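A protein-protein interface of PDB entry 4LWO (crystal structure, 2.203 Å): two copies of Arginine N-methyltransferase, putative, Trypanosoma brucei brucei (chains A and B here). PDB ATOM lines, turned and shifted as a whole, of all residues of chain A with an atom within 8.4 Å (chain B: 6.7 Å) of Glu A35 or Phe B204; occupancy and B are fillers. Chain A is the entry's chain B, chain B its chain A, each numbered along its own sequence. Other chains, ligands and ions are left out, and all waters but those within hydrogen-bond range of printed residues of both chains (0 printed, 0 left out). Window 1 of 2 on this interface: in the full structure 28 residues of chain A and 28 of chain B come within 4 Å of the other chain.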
ATOM      1  N   LEU A  27     -23.581  30.400  12.802  1.00  0.00           N
ATOM      2  CA  LEU A  27     -22.865  29.298  13.442  1.00  0.00           C
ATOM      3  C   LEU A  27     -22.798  29.410  14.959  1.00  0.00           C
ATOM      4  O   LEU A  27     -22.691  28.404  15.669  1.00  0.00           O
ATOM      5  CB  LEU A  27     -21.439  29.239  12.901  1.00  0.00           C
ATOM      6  CG  LEU A  27     -21.115  28.216  11.819  1.00  0.00           C
ATOM      7  CD1 LEU A  27     -19.658  28.325  11.423  1.00  0.00           C
ATOM      8  CD2 LEU A  27     -21.426  26.827  12.318  1.00  0.00           C
ATOM      9  N   ALA A  28     -22.823  30.642  15.454  1.00  0.00           N
ATOM     10  CA  ALA A  28     -22.698  30.871  16.884  1.00  0.00           C
ATOM     11  C   ALA A  28     -23.845  30.170  17.600  1.00  0.00           C
ATOM     12  O   ALA A  28     -23.637  29.427  18.561  1.00  0.00           O
ATOM     13  CB  ALA A  28     -22.699  32.361  17.185  1.00  0.00           C
ATOM     14  N   VAL A  29     -25.055  30.400  17.105  1.00  0.00           N
ATOM     15  CA  VAL A  29     -26.245  29.771  17.655  1.00  0.00           C
ATOM     16  C   VAL A  29     -26.146  28.228  17.661  1.00  0.00           C
ATOM     17  O   VAL A  29     -26.338  27.589  18.702  1.00  0.00           O
ATOM     18  CB  VAL A  29     -27.530  30.303  16.938  1.00  0.00           C
ATOM     19  CG1 VAL A  29     -28.337  29.185  16.264  1.00  0.00           C
ATOM     20  CG2 VAL A  29     -28.393  31.080  17.921  1.00  0.00           C
ATOM     21  N   HIS A  30     -25.798  27.638  16.520  1.00  0.00           N
ATOM     22  CA  HIS A  30     -25.827  26.192  16.398  1.00  0.00           C
ATOM     23  C   HIS A  30     -24.776  25.553  17.297  1.00  0.00           C
ATOM     24  O   HIS A  30     -24.947  24.427  17.763  1.00  0.00           O
ATOM     25  CB  HIS A  30     -25.685  25.779  14.944  1.00  0.00           C
ATOM     26  CG  HIS A  30     -26.823  26.233  14.080  1.00  0.00           C
ATOM     27  ND1 HIS A  30     -28.102  25.733  14.212  1.00  0.00           N
ATOM     28  CD2 HIS A  30     -26.878  27.136  13.072  1.00  0.00           C
ATOM     29  CE1 HIS A  30     -28.895  26.311  13.326  1.00  0.00           C
ATOM     30  NE2 HIS A  30     -28.177  27.166  12.620  1.00  0.00           N
ATOM     31  N   ARG A  31     -23.705  26.289  17.569  1.00  0.00           N
ATOM     32  CA  ARG A  31     -22.729  25.844  18.549  1.00  0.00           C
ATOM     33  C   ARG A  31     -23.401  25.572  19.907  1.00  0.00           C
ATOM     34  O   ARG A  31     -23.093  24.570  20.571  1.00  0.00           O
ATOM     35  CB  ARG A  31     -21.608  26.877  18.688  1.00  0.00           C
ATOM     36  CG  ARG A  31     -20.538  26.480  19.682  1.00  0.00           C
ATOM     37  CD  ARG A  31     -19.184  27.127  19.372  1.00  0.00           C
ATOM     38  NE  ARG A  31     -18.192  26.750  20.376  1.00  0.00           N
ATOM     39  CZ  ARG A  31     -16.878  26.921  20.250  1.00  0.00           C
ATOM     40  NH1 ARG A  31     -16.365  27.457  19.152  1.00  0.00           N
ATOM     41  NH2 ARG A  31     -16.072  26.544  21.228  1.00  0.00           N
ATOM     42  N   LEU A  32     -24.327  26.451  20.302  1.00  0.00           N
ATOM     43  CA  LEU A  32     -25.045  26.313  21.580  1.00  0.00           C
ATOM     44  C   LEU A  32     -25.874  25.021  21.668  1.00  0.00           C
ATOM     45  O   LEU A  32     -25.914  24.372  22.715  1.00  0.00           O
ATOM     46  CB  LEU A  32     -25.948  27.525  21.843  1.00  0.00           C
ATOM     47  CG  LEU A  32     -25.362  28.930  21.994  1.00  0.00           C
ATOM     48  CD1 LEU A  32     -26.477  29.909  22.349  1.00  0.00           C
ATOM     49  CD2 LEU A  32     -24.241  28.977  23.035  1.00  0.00           C
ATOM     50  N   MET A  33     -26.549  24.675  20.574  1.00  0.00           N
ATOM     51  CA  MET A  33     -27.202  23.372  20.427  1.00  0.00           C
ATOM     52  C   MET A  33     -26.173  22.268  20.662  1.00  0.00           C
ATOM     53  O   MET A  33     -26.361  21.378  21.492  1.00  0.00           O
ATOM     54  CB  MET A  33     -27.774  23.250  19.010  1.00  0.00           C
ATOM     55  CG  MET A  33     -28.672  22.040  18.728  1.00  0.00           C
ATOM     56  SD  MET A  33     -27.878  20.422  18.660  1.00  0.00           S
ATOM     57  CE  MET A  33     -29.202  19.410  18.002  1.00  0.00           C
ATOM     58  N   LEU A  34     -25.075  22.338  19.919  1.00  0.00           N
ATOM     59  CA  LEU A  34     -23.991  21.368  20.040  1.00  0.00           C
ATOM     60  C   LEU A  34     -23.343  21.391  21.424  1.00  0.00           C
ATOM     61  O   LEU A  34     -22.772  20.402  21.857  1.00  0.00           O
ATOM     62  CB  LEU A  34     -22.954  21.603  18.943  1.00  0.00           C
ATOM     63  CG  LEU A  34     -23.553  21.446  17.539  1.00  0.00           C
ATOM     64  CD1 LEU A  34     -22.564  21.830  16.455  1.00  0.00           C
ATOM     65  CD2 LEU A  34     -24.072  20.030  17.301  1.00  0.00           C
ATOM     66  N   GLU A  35     -23.460  22.509  22.133  1.00  0.00           N
ATOM     67  CA  GLU A  35     -22.883  22.586  23.473  1.00  0.00           C
ATOM     68  C   GLU A  35     -23.841  22.147  24.576  1.00  0.00           C
ATOM     69  O   GLU A  35     -23.463  22.066  25.738  1.00  0.00           O
ATOM     70  CB  GLU A  35     -22.365  23.989  23.754  1.00  0.00           C
ATOM     71  CG  GLU A  35     -20.844  24.062  23.789  1.00  0.00           C
ATOM     72  CD  GLU A  35     -20.309  25.401  23.308  1.00  0.00           C
ATOM     73  OE1 GLU A  35     -21.092  26.383  23.283  1.00  0.00           O
ATOM     74  OE2 GLU A  35     -19.108  25.459  22.943  1.00  0.00           O
ATOM     75  N   ASP A  36     -25.082  21.853  24.213  1.00  0.00           N
ATOM     76  CA  ASP A  36     -26.060  21.463  25.212  1.00  0.00           C
ATOM     77  C   ASP A  36     -26.224  19.949  25.226  1.00  0.00           C
ATOM     78  O   ASP A  36     -26.802  19.355  24.296  1.00  0.00           O
ATOM     79  CB  ASP A  36     -27.389  22.147  24.923  1.00  0.00           C
ATOM     80  CG  ASP A  36     -28.393  21.978  26.047  1.00  0.00           C
ATOM     81  OD1 ASP A  36     -28.653  20.827  26.456  1.00  0.00           O
ATOM     82  OD2 ASP A  36     -28.939  23.008  26.499  1.00  0.00           O
ATOM     83  N   ALA A  37     -25.726  19.327  26.292  1.00  0.00           N
ATOM     84  CA  ALA A  37     -25.788  17.872  26.422  1.00  0.00           C
ATOM     85  C   ALA A  37     -27.228  17.330  26.375  1.00  0.00           C
ATOM     86  O   ALA A  37     -27.470  16.259  25.817  1.00  0.00           O
ATOM     87  CB  ALA A  37     -25.080  17.414  27.710  1.00  0.00           C
ATOM     88  N   GLN A  38     -28.172  18.064  26.966  1.00  0.00           N
ATOM     89  CA  GLN A  38     -29.555  17.600  27.053  1.00  0.00           C
ATOM     90  C   GLN A  38     -30.146  17.542  25.645  1.00  0.00           C
ATOM     91  O   GLN A  38     -30.691  16.529  25.243  1.00  0.00           O
ATOM     92  CB  GLN A  38     -30.394  18.523  27.959  1.00  0.00           C
ATOM     93  CG  GLN A  38     -31.289  17.777  28.965  1.00  0.00           C
ATOM     94  CD  GLN A  38     -32.572  18.550  29.369  1.00  0.00           C
ATOM     95  OE1 GLN A  38     -33.691  17.993  29.337  1.00  0.00           O
ATOM     96  NE2 GLN A  38     -32.407  19.820  29.775  1.00  0.00           N
ATOM     97  N   ARG A  39     -30.026  18.639  24.902  1.00  0.00           N
ATOM     98  CA  ARG A  39     -30.541  18.700  23.542  1.00  0.00           C
ATOM     99  C   ARG A  39     -29.929  17.632  22.632  1.00  0.00           C
ATOM    100  O   ARG A  39     -30.657  16.880  21.965  1.00  0.00           O
ATOM    101  CB  ARG A  39     -30.339  20.098  22.964  1.00  0.00           C
ATOM    102  CG  ARG A  39     -31.365  21.108  23.458  1.00  0.00           C
ATOM    103  CD  ARG A  39     -30.699  22.443  23.804  1.00  0.00           C
ATOM    104  NE  ARG A  39     -30.906  23.566  22.881  1.00  0.00           N
ATOM    105  CZ  ARG A  39     -30.802  23.512  21.555  1.00  0.00           C
ATOM    106  NH1 ARG A  39     -30.981  24.600  20.809  1.00  0.00           N
ATOM    107  NH2 ARG A  39     -30.518  22.376  20.967  1.00  0.00           N
ATOM    108  N   MET A  40     -28.597  17.563  22.622  1.00  0.00           N
ATOM    109  CA  MET A  40     -27.862  16.577  21.832  1.00  0.00           C
ATOM    110  C   MET A  40     -28.352  15.189  22.174  1.00  0.00           C
ATOM    111  O   MET A  40     -28.643  14.387  21.288  1.00  0.00           O
ATOM    112  CB  MET A  40     -26.355  16.659  22.128  1.00  0.00           C
ATOM    113  CG  MET A  40     -25.691  17.924  21.610  1.00  0.00           C
ATOM    114  SD  MET A  40     -25.603  17.928  19.808  1.00  0.00           S
ATOM    115  CE  MET A  40     -24.321  16.683  19.572  1.00  0.00           C
ATOM    116  N   THR A  65     -26.262  22.891  11.310  1.00  0.00           N
ATOM    117  CA  THR A  65     -25.014  22.179  11.093  1.00  0.00           C
ATOM    118  C   THR A  65     -25.238  20.836  10.377  1.00  0.00           C
ATOM    119  O   THR A  65     -24.283  20.222   9.906  1.00  0.00           O
ATOM    120  CB  THR A  65     -24.316  21.888  12.421  1.00  0.00           C
ATOM    121  OG1 THR A  65     -25.255  21.264  13.303  1.00  0.00           O
ATOM    122  CG2 THR A  65     -23.793  23.182  13.069  1.00  0.00           C
ATOM    123  N   SER A 316     -30.010  23.905  32.730  1.00  0.00           N
ATOM    124  CA  SER A 316     -30.327  25.114  31.989  1.00  0.00           C
ATOM    125  C   SER A 316     -30.156  24.878  30.490  1.00  0.00           C
ATOM    126  O   SER A 316     -29.341  24.047  30.068  1.00  0.00           O
ATOM    127  CB  SER A 316     -29.399  26.242  32.455  1.00  0.00           C
ATOM    128  OG  SER A 316     -29.575  27.419  31.691  1.00  0.00           O
ATOM    129  N   VAL B 198      -6.885  27.023  18.429  1.00  0.00           N
ATOM    130  CA  VAL B 198      -6.873  25.660  18.946  1.00  0.00           C
ATOM    131  C   VAL B 198      -7.850  25.536  20.118  1.00  0.00           C
ATOM    132  O   VAL B 198      -8.803  24.746  20.072  1.00  0.00           O
ATOM    133  CB  VAL B 198      -5.440  25.197  19.350  1.00  0.00           C
ATOM    134  CG1 VAL B 198      -5.491  23.984  20.263  1.00  0.00           C
ATOM    135  CG2 VAL B 198      -4.588  24.897  18.111  1.00  0.00           C
ATOM    136  N   GLN B 199      -7.634  26.345  21.145  1.00  0.00           N
ATOM    137  CA  GLN B 199      -8.403  26.236  22.378  1.00  0.00           C
ATOM    138  C   GLN B 199      -9.863  26.630  22.239  1.00  0.00           C
ATOM    139  O   GLN B 199     -10.709  26.039  22.900  1.00  0.00           O
ATOM    140  CB  GLN B 199      -7.743  27.040  23.502  1.00  0.00           C
ATOM    141  CG  GLN B 199      -6.376  26.474  23.937  1.00  0.00           C
ATOM    142  CD  GLN B 199      -5.572  27.450  24.789  1.00  0.00           C
ATOM    143  OE1 GLN B 199      -6.089  28.041  25.745  1.00  0.00           O
ATOM    144  NE2 GLN B 199      -4.303  27.631  24.436  1.00  0.00           N
ATOM    145  N   ARG B 200     -10.166  27.623  21.404  1.00  0.00           N
ATOM    146  CA  ARG B 200     -11.543  28.112  21.309  1.00  0.00           C
ATOM    147  C   ARG B 200     -12.379  27.482  20.191  1.00  0.00           C
ATOM    148  O   ARG B 200     -13.598  27.412  20.312  1.00  0.00           O
ATOM    149  CB  ARG B 200     -11.593  29.643  21.200  1.00  0.00           C
ATOM    150  N   TYR B 201     -11.735  27.023  19.117  1.00  0.00           N
ATOM    151  CA  TYR B 201     -12.467  26.500  17.964  1.00  0.00           C
ATOM    152  C   TYR B 201     -12.159  25.055  17.588  1.00  0.00           C
ATOM    153  O   TYR B 201     -13.058  24.210  17.518  1.00  0.00           O
ATOM    154  CB  TYR B 201     -12.237  27.404  16.749  1.00  0.00           C
ATOM    155  CG  TYR B 201     -12.691  28.818  17.008  1.00  0.00           C
ATOM    156  CD1 TYR B 201     -11.832  29.748  17.572  1.00  0.00           C
ATOM    157  CD2 TYR B 201     -13.996  29.211  16.729  1.00  0.00           C
ATOM    158  CE1 TYR B 201     -12.252  31.032  17.839  1.00  0.00           C
ATOM    159  CE2 TYR B 201     -14.423  30.493  16.983  1.00  0.00           C
ATOM    160  CZ  TYR B 201     -13.551  31.399  17.539  1.00  0.00           C
ATOM    161  OH  TYR B 201     -13.977  32.675  17.798  1.00  0.00           O
ATOM    162  N   LYS B 202     -10.889  24.781  17.335  1.00  0.00           N
ATOM    163  CA  LYS B 202     -10.462  23.528  16.716  1.00  0.00           C
ATOM    164  C   LYS B 202     -10.774  22.283  17.552  1.00  0.00           C
ATOM    165  O   LYS B 202     -11.170  21.247  17.006  1.00  0.00           O
ATOM    166  CB  LYS B 202      -8.968  23.587  16.400  1.00  0.00           C
ATOM    167  CG  LYS B 202      -8.519  22.619  15.326  1.00  0.00           C
ATOM    168  CD  LYS B 202      -7.755  21.447  15.906  1.00  0.00           C
ATOM    169  CE  LYS B 202      -6.322  21.429  15.401  1.00  0.00           C
ATOM    170  NZ  LYS B 202      -6.280  21.498  13.918  1.00  0.00           N
ATOM    171  N   ASN B 203     -10.589  22.392  18.864  1.00  0.00           N
ATOM    172  CA  ASN B 203     -10.844  21.280  19.774  1.00  0.00           C
ATOM    173  C   ASN B 203     -12.327  20.990  20.014  1.00  0.00           C
ATOM    174  O   ASN B 203     -12.698  19.853  20.283  1.00  0.00           O
ATOM    175  CB  ASN B 203     -10.148  21.516  21.112  1.00  0.00           C
ATOM    176  CG  ASN B 203      -8.667  21.180  21.068  1.00  0.00           C
ATOM    177  OD1 ASN B 203      -8.128  20.783  20.029  1.00  0.00           O
ATOM    178  ND2 ASN B 203      -8.002  21.344  22.200  1.00  0.00           N
ATOM    179  N   PHE B 204     -13.171  22.016  19.950  1.00  0.00           N
ATOM    180  CA  PHE B 204     -14.610  21.795  20.058  1.00  0.00           C
ATOM    181  C   PHE B 204     -15.149  21.146  18.787  1.00  0.00           C
ATOM    182  O   PHE B 204     -15.909  20.185  18.835  1.00  0.00           O
ATOM    183  CB  PHE B 204     -15.360  23.106  20.300  1.00  0.00           C
ATOM    184  CG  PHE B 204     -16.854  22.963  20.192  1.00  0.00           C
ATOM    185  CD1 PHE B 204     -17.586  22.411  21.234  1.00  0.00           C
ATOM    186  CD2 PHE B 204     -17.521  23.350  19.040  1.00  0.00           C
ATOM    187  CE1 PHE B 204     -18.959  22.261  21.136  1.00  0.00           C
ATOM    188  CE2 PHE B 204     -18.894  23.199  18.931  1.00  0.00           C
ATOM    189  CZ  PHE B 204     -19.614  22.660  19.981  1.00  0.00           C
ATOM    190  N   TRP B 205     -14.741  21.691  17.650  1.00  0.00           N
ATOM    191  CA  TRP B 205     -15.317  21.342  16.366  1.00  0.00           C
ATOM    192  C   TRP B 205     -14.708  20.098  15.716  1.00  0.00           C
ATOM    193  O   TRP B 205     -15.210  19.645  14.682  1.00  0.00           O
ATOM    194  CB  TRP B 205     -15.176  22.524  15.405  1.00  0.00           C
ATOM    195  CG  TRP B 205     -16.114  23.701  15.643  1.00  0.00           C
ATOM    196  CD1 TRP B 205     -15.775  24.944  16.089  1.00  0.00           C
ATOM    197  CD2 TRP B 205     -17.530  23.739  15.402  1.00  0.00           C
ATOM    198  NE1 TRP B 205     -16.889  25.755  16.146  1.00  0.00           N
ATOM    199  CE2 TRP B 205     -17.979  25.035  15.733  1.00  0.00           C
ATOM    200  CE3 TRP B 205     -18.458  22.800  14.959  1.00  0.00           C
ATOM    201  CZ2 TRP B 205     -19.316  25.412  15.622  1.00  0.00           C
ATOM    202  CZ3 TRP B 205     -19.783  23.179  14.847  1.00  0.00           C
ATOM    203  CH2 TRP B 205     -20.199  24.471  15.172  1.00  0.00           C
ATOM    204  N   ARG B 206     -13.631  19.555  16.296  1.00  0.00           N
ATOM    205  CA  ARG B 206     -12.934  18.429  15.672  1.00  0.00           C
ATOM    206  C   ARG B 206     -13.783  17.167  15.714  1.00  0.00           C
ATOM    207  O   ARG B 206     -13.824  16.400  14.750  1.00  0.00           O
ATOM    208  CB  ARG B 206     -11.551  18.166  16.307  1.00  0.00           C
ATOM    209  CG  ARG B 206     -11.582  17.689  17.774  1.00  0.00           C
ATOM    210  CD  ARG B 206     -10.252  17.062  18.238  1.00  0.00           C
ATOM    211  NE  ARG B 206      -9.943  15.793  17.569  1.00  0.00           N
ATOM    212  CZ  ARG B 206     -10.281  14.583  18.027  1.00  0.00           C
ATOM    213  NH1 ARG B 206     -10.956  14.445  19.165  1.00  0.00           N
ATOM    214  NH2 ARG B 206      -9.943  13.498  17.340  1.00  0.00           N
ATOM    215  N   ASP B 207     -14.447  16.952  16.844  1.00  0.00           N
ATOM    216  CA  ASP B 207     -15.254  15.764  17.023  1.00  0.00           C
ATOM    217  C   ASP B 207     -16.583  16.081  17.680  1.00  0.00           C
ATOM    218  O   ASP B 207     -16.644  16.384  18.872  1.00  0.00           O
ATOM    219  CB  ASP B 207     -14.528  14.724  17.855  1.00  0.00           C
ATOM    220  CG  ASP B 207     -15.260  13.406  17.874  1.00  0.00           C
ATOM    221  OD1 ASP B 207     -16.163  13.236  18.724  1.00  0.00           O
ATOM    222  OD2 ASP B 207     -14.952  12.558  17.009  1.00  0.00           O
ATOM    223  N   VAL B 208     -17.643  16.012  16.882  1.00  0.00           N
ATOM    224  CA  VAL B 208     -19.002  16.127  17.383  1.00  0.00           C
ATOM    225  C   VAL B 208     -19.648  14.755  17.211  1.00  0.00           C
ATOM    226  O   VAL B 208     -20.046  14.390  16.097  1.00  0.00           O
ATOM    227  CB  VAL B 208     -19.798  17.182  16.596  1.00  0.00           C
ATOM    228  CG1 VAL B 208     -21.099  17.498  17.306  1.00  0.00           C
ATOM    229  CG2 VAL B 208     -18.972  18.448  16.426  1.00  0.00           C
ATOM    230  N   PHE B 213     -16.362  18.039  12.264  1.00  0.00           N
ATOM    231  CA  PHE B 213     -16.984  19.327  11.979  1.00  0.00           C
ATOM    232  C   PHE B 213     -15.931  20.437  11.911  1.00  0.00           C
ATOM    233  O   PHE B 213     -16.259  21.610  12.120  1.00  0.00           O
ATOM    234  CB  PHE B 213     -18.033  19.679  13.059  1.00  0.00           C
ATOM    235  CG  PHE B 213     -19.427  19.092  12.809  1.00  0.00           C
ATOM    236  CD1 PHE B 213     -19.606  17.979  11.988  1.00  0.00           C
ATOM    237  CD2 PHE B 213     -20.554  19.677  13.396  1.00  0.00           C
ATOM    238  CE1 PHE B 213     -20.898  17.449  11.759  1.00  0.00           C
ATOM    239  CE2 PHE B 213     -21.836  19.165  13.175  1.00  0.00           C
ATOM    240  CZ  PHE B 213     -22.013  18.044  12.360  1.00  0.00           C
ATOM    241  N   GLU B 220     -16.024  29.692  11.670  1.00  0.00           N
ATOM    242  CA  GLU B 220     -16.398  30.476  12.845  1.00  0.00           C
ATOM    243  C   GLU B 220     -15.239  31.404  13.244  1.00  0.00           C
ATOM    244  O   GLU B 220     -15.444  32.567  13.585  1.00  0.00           O
ATOM    245  CB  GLU B 220     -16.760  29.541  14.006  1.00  0.00           C
ATOM    246  CG  GLU B 220     -17.663  30.165  15.083  1.00  0.00           C
ATOM    247  CD  GLU B 220     -17.641  29.397  16.409  1.00  0.00           C
ATOM    248  OE1 GLU B 220     -17.156  28.246  16.438  1.00  0.00           O
ATOM    249  OE2 GLU B 220     -18.094  29.952  17.432  1.00  0.00           O
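NH2 of Arg A31 is in hydrogen-bond range of O of Arg B200 (2.8 Å). The guanidinium group of Arg A31 lies within salt-bridge range of the side-chain carboxylate of Glu B220 (2.9 Å). NE1 of Trp B205 lies close to NH1 of Arg A31, at 3.5 Å.
No position is printed for both chains. Of the 12 pairs that touch across the chains among the printed residues, none has its exchanged pair printed and touching as well.
Printed residues of chain B that touch a printed residue of chain A: Arg B200, Tyr B201, Phe B204, Trp B205, Val B208, Phe B213 and Glu B220. Hydrophobic or aromatic side chains of chain B within 4 Å of the printed part of chain A: Tyr B201, Phe B204, Trp B205, Val B208 and Phe B213. Hydrophobic or aromatic side chains of chain A within 4 Å of the printed part of chain B: Leu A27 and Leu A34. Among the printed residues, Asp or Glu carboxylates within 4 Å of a Lys or Arg side-chain nitrogen of the other chain: Arg A31 with Glu B220 (2.9 Å).
Of chain B, only Phe B204 (3.7 Å) comes within 4 Å of Glu A35. Of chain A, only Arg A31, Leu A34 and Glu A35 come within 4 Å of Phe B204. Printed residues of chain A within 4 Å of Trp B205: Leu A27 (3.9 Å), Arg A31 (3.5 Å) and Leu A34 (3.5 Å). Of the printed residues of chain B, Thr A65 touches Phe B213. Of the printed residues of chain A, Glu B220 touches Leu A27 and Arg A31. Of the printed residues of chain B, Arg A31 touches Arg B200, Tyr B201, Phe B204, Trp B205 and Glu B220. Asp A36 touches none of the printed residues of chain B. Arg A39 touches none of the printed residues of chain B. The nearest residue of chain B that does not touch Glu A35 is Arg B200 (6.4 Å).
Among the printed residues, pairs that only touch across the chains: Leu A27 with Trp B205 (3.9 Å), Leu A27 with Glu B220 (3.9 Å), Arg A31 with Tyr B201 (3.8 Å), Arg A31 with Phe B204 (3.6 Å), Leu A34 with Phe B204 (3.7 Å), Leu A34 with Trp B205 (3.5 Å), Leu A34 with Val B208 (3.9 Å), Glu A35 with Phe B204 (3.7 Å) and Thr A65 with Phe B213 (3.8 Å).
NE of Arg A31 lies within salt-bridge range of OE2 of Glu A35 (3.0 Å). The backbone carbonyl oxygen of Trp B205 lies close to the backbone NH of Phe B213. The side-chain carboxylate (OE1) of Glu B220 is in hydrogen-bond range of the indole nitrogen (NE1) of Trp B205, at 2.5 Å.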
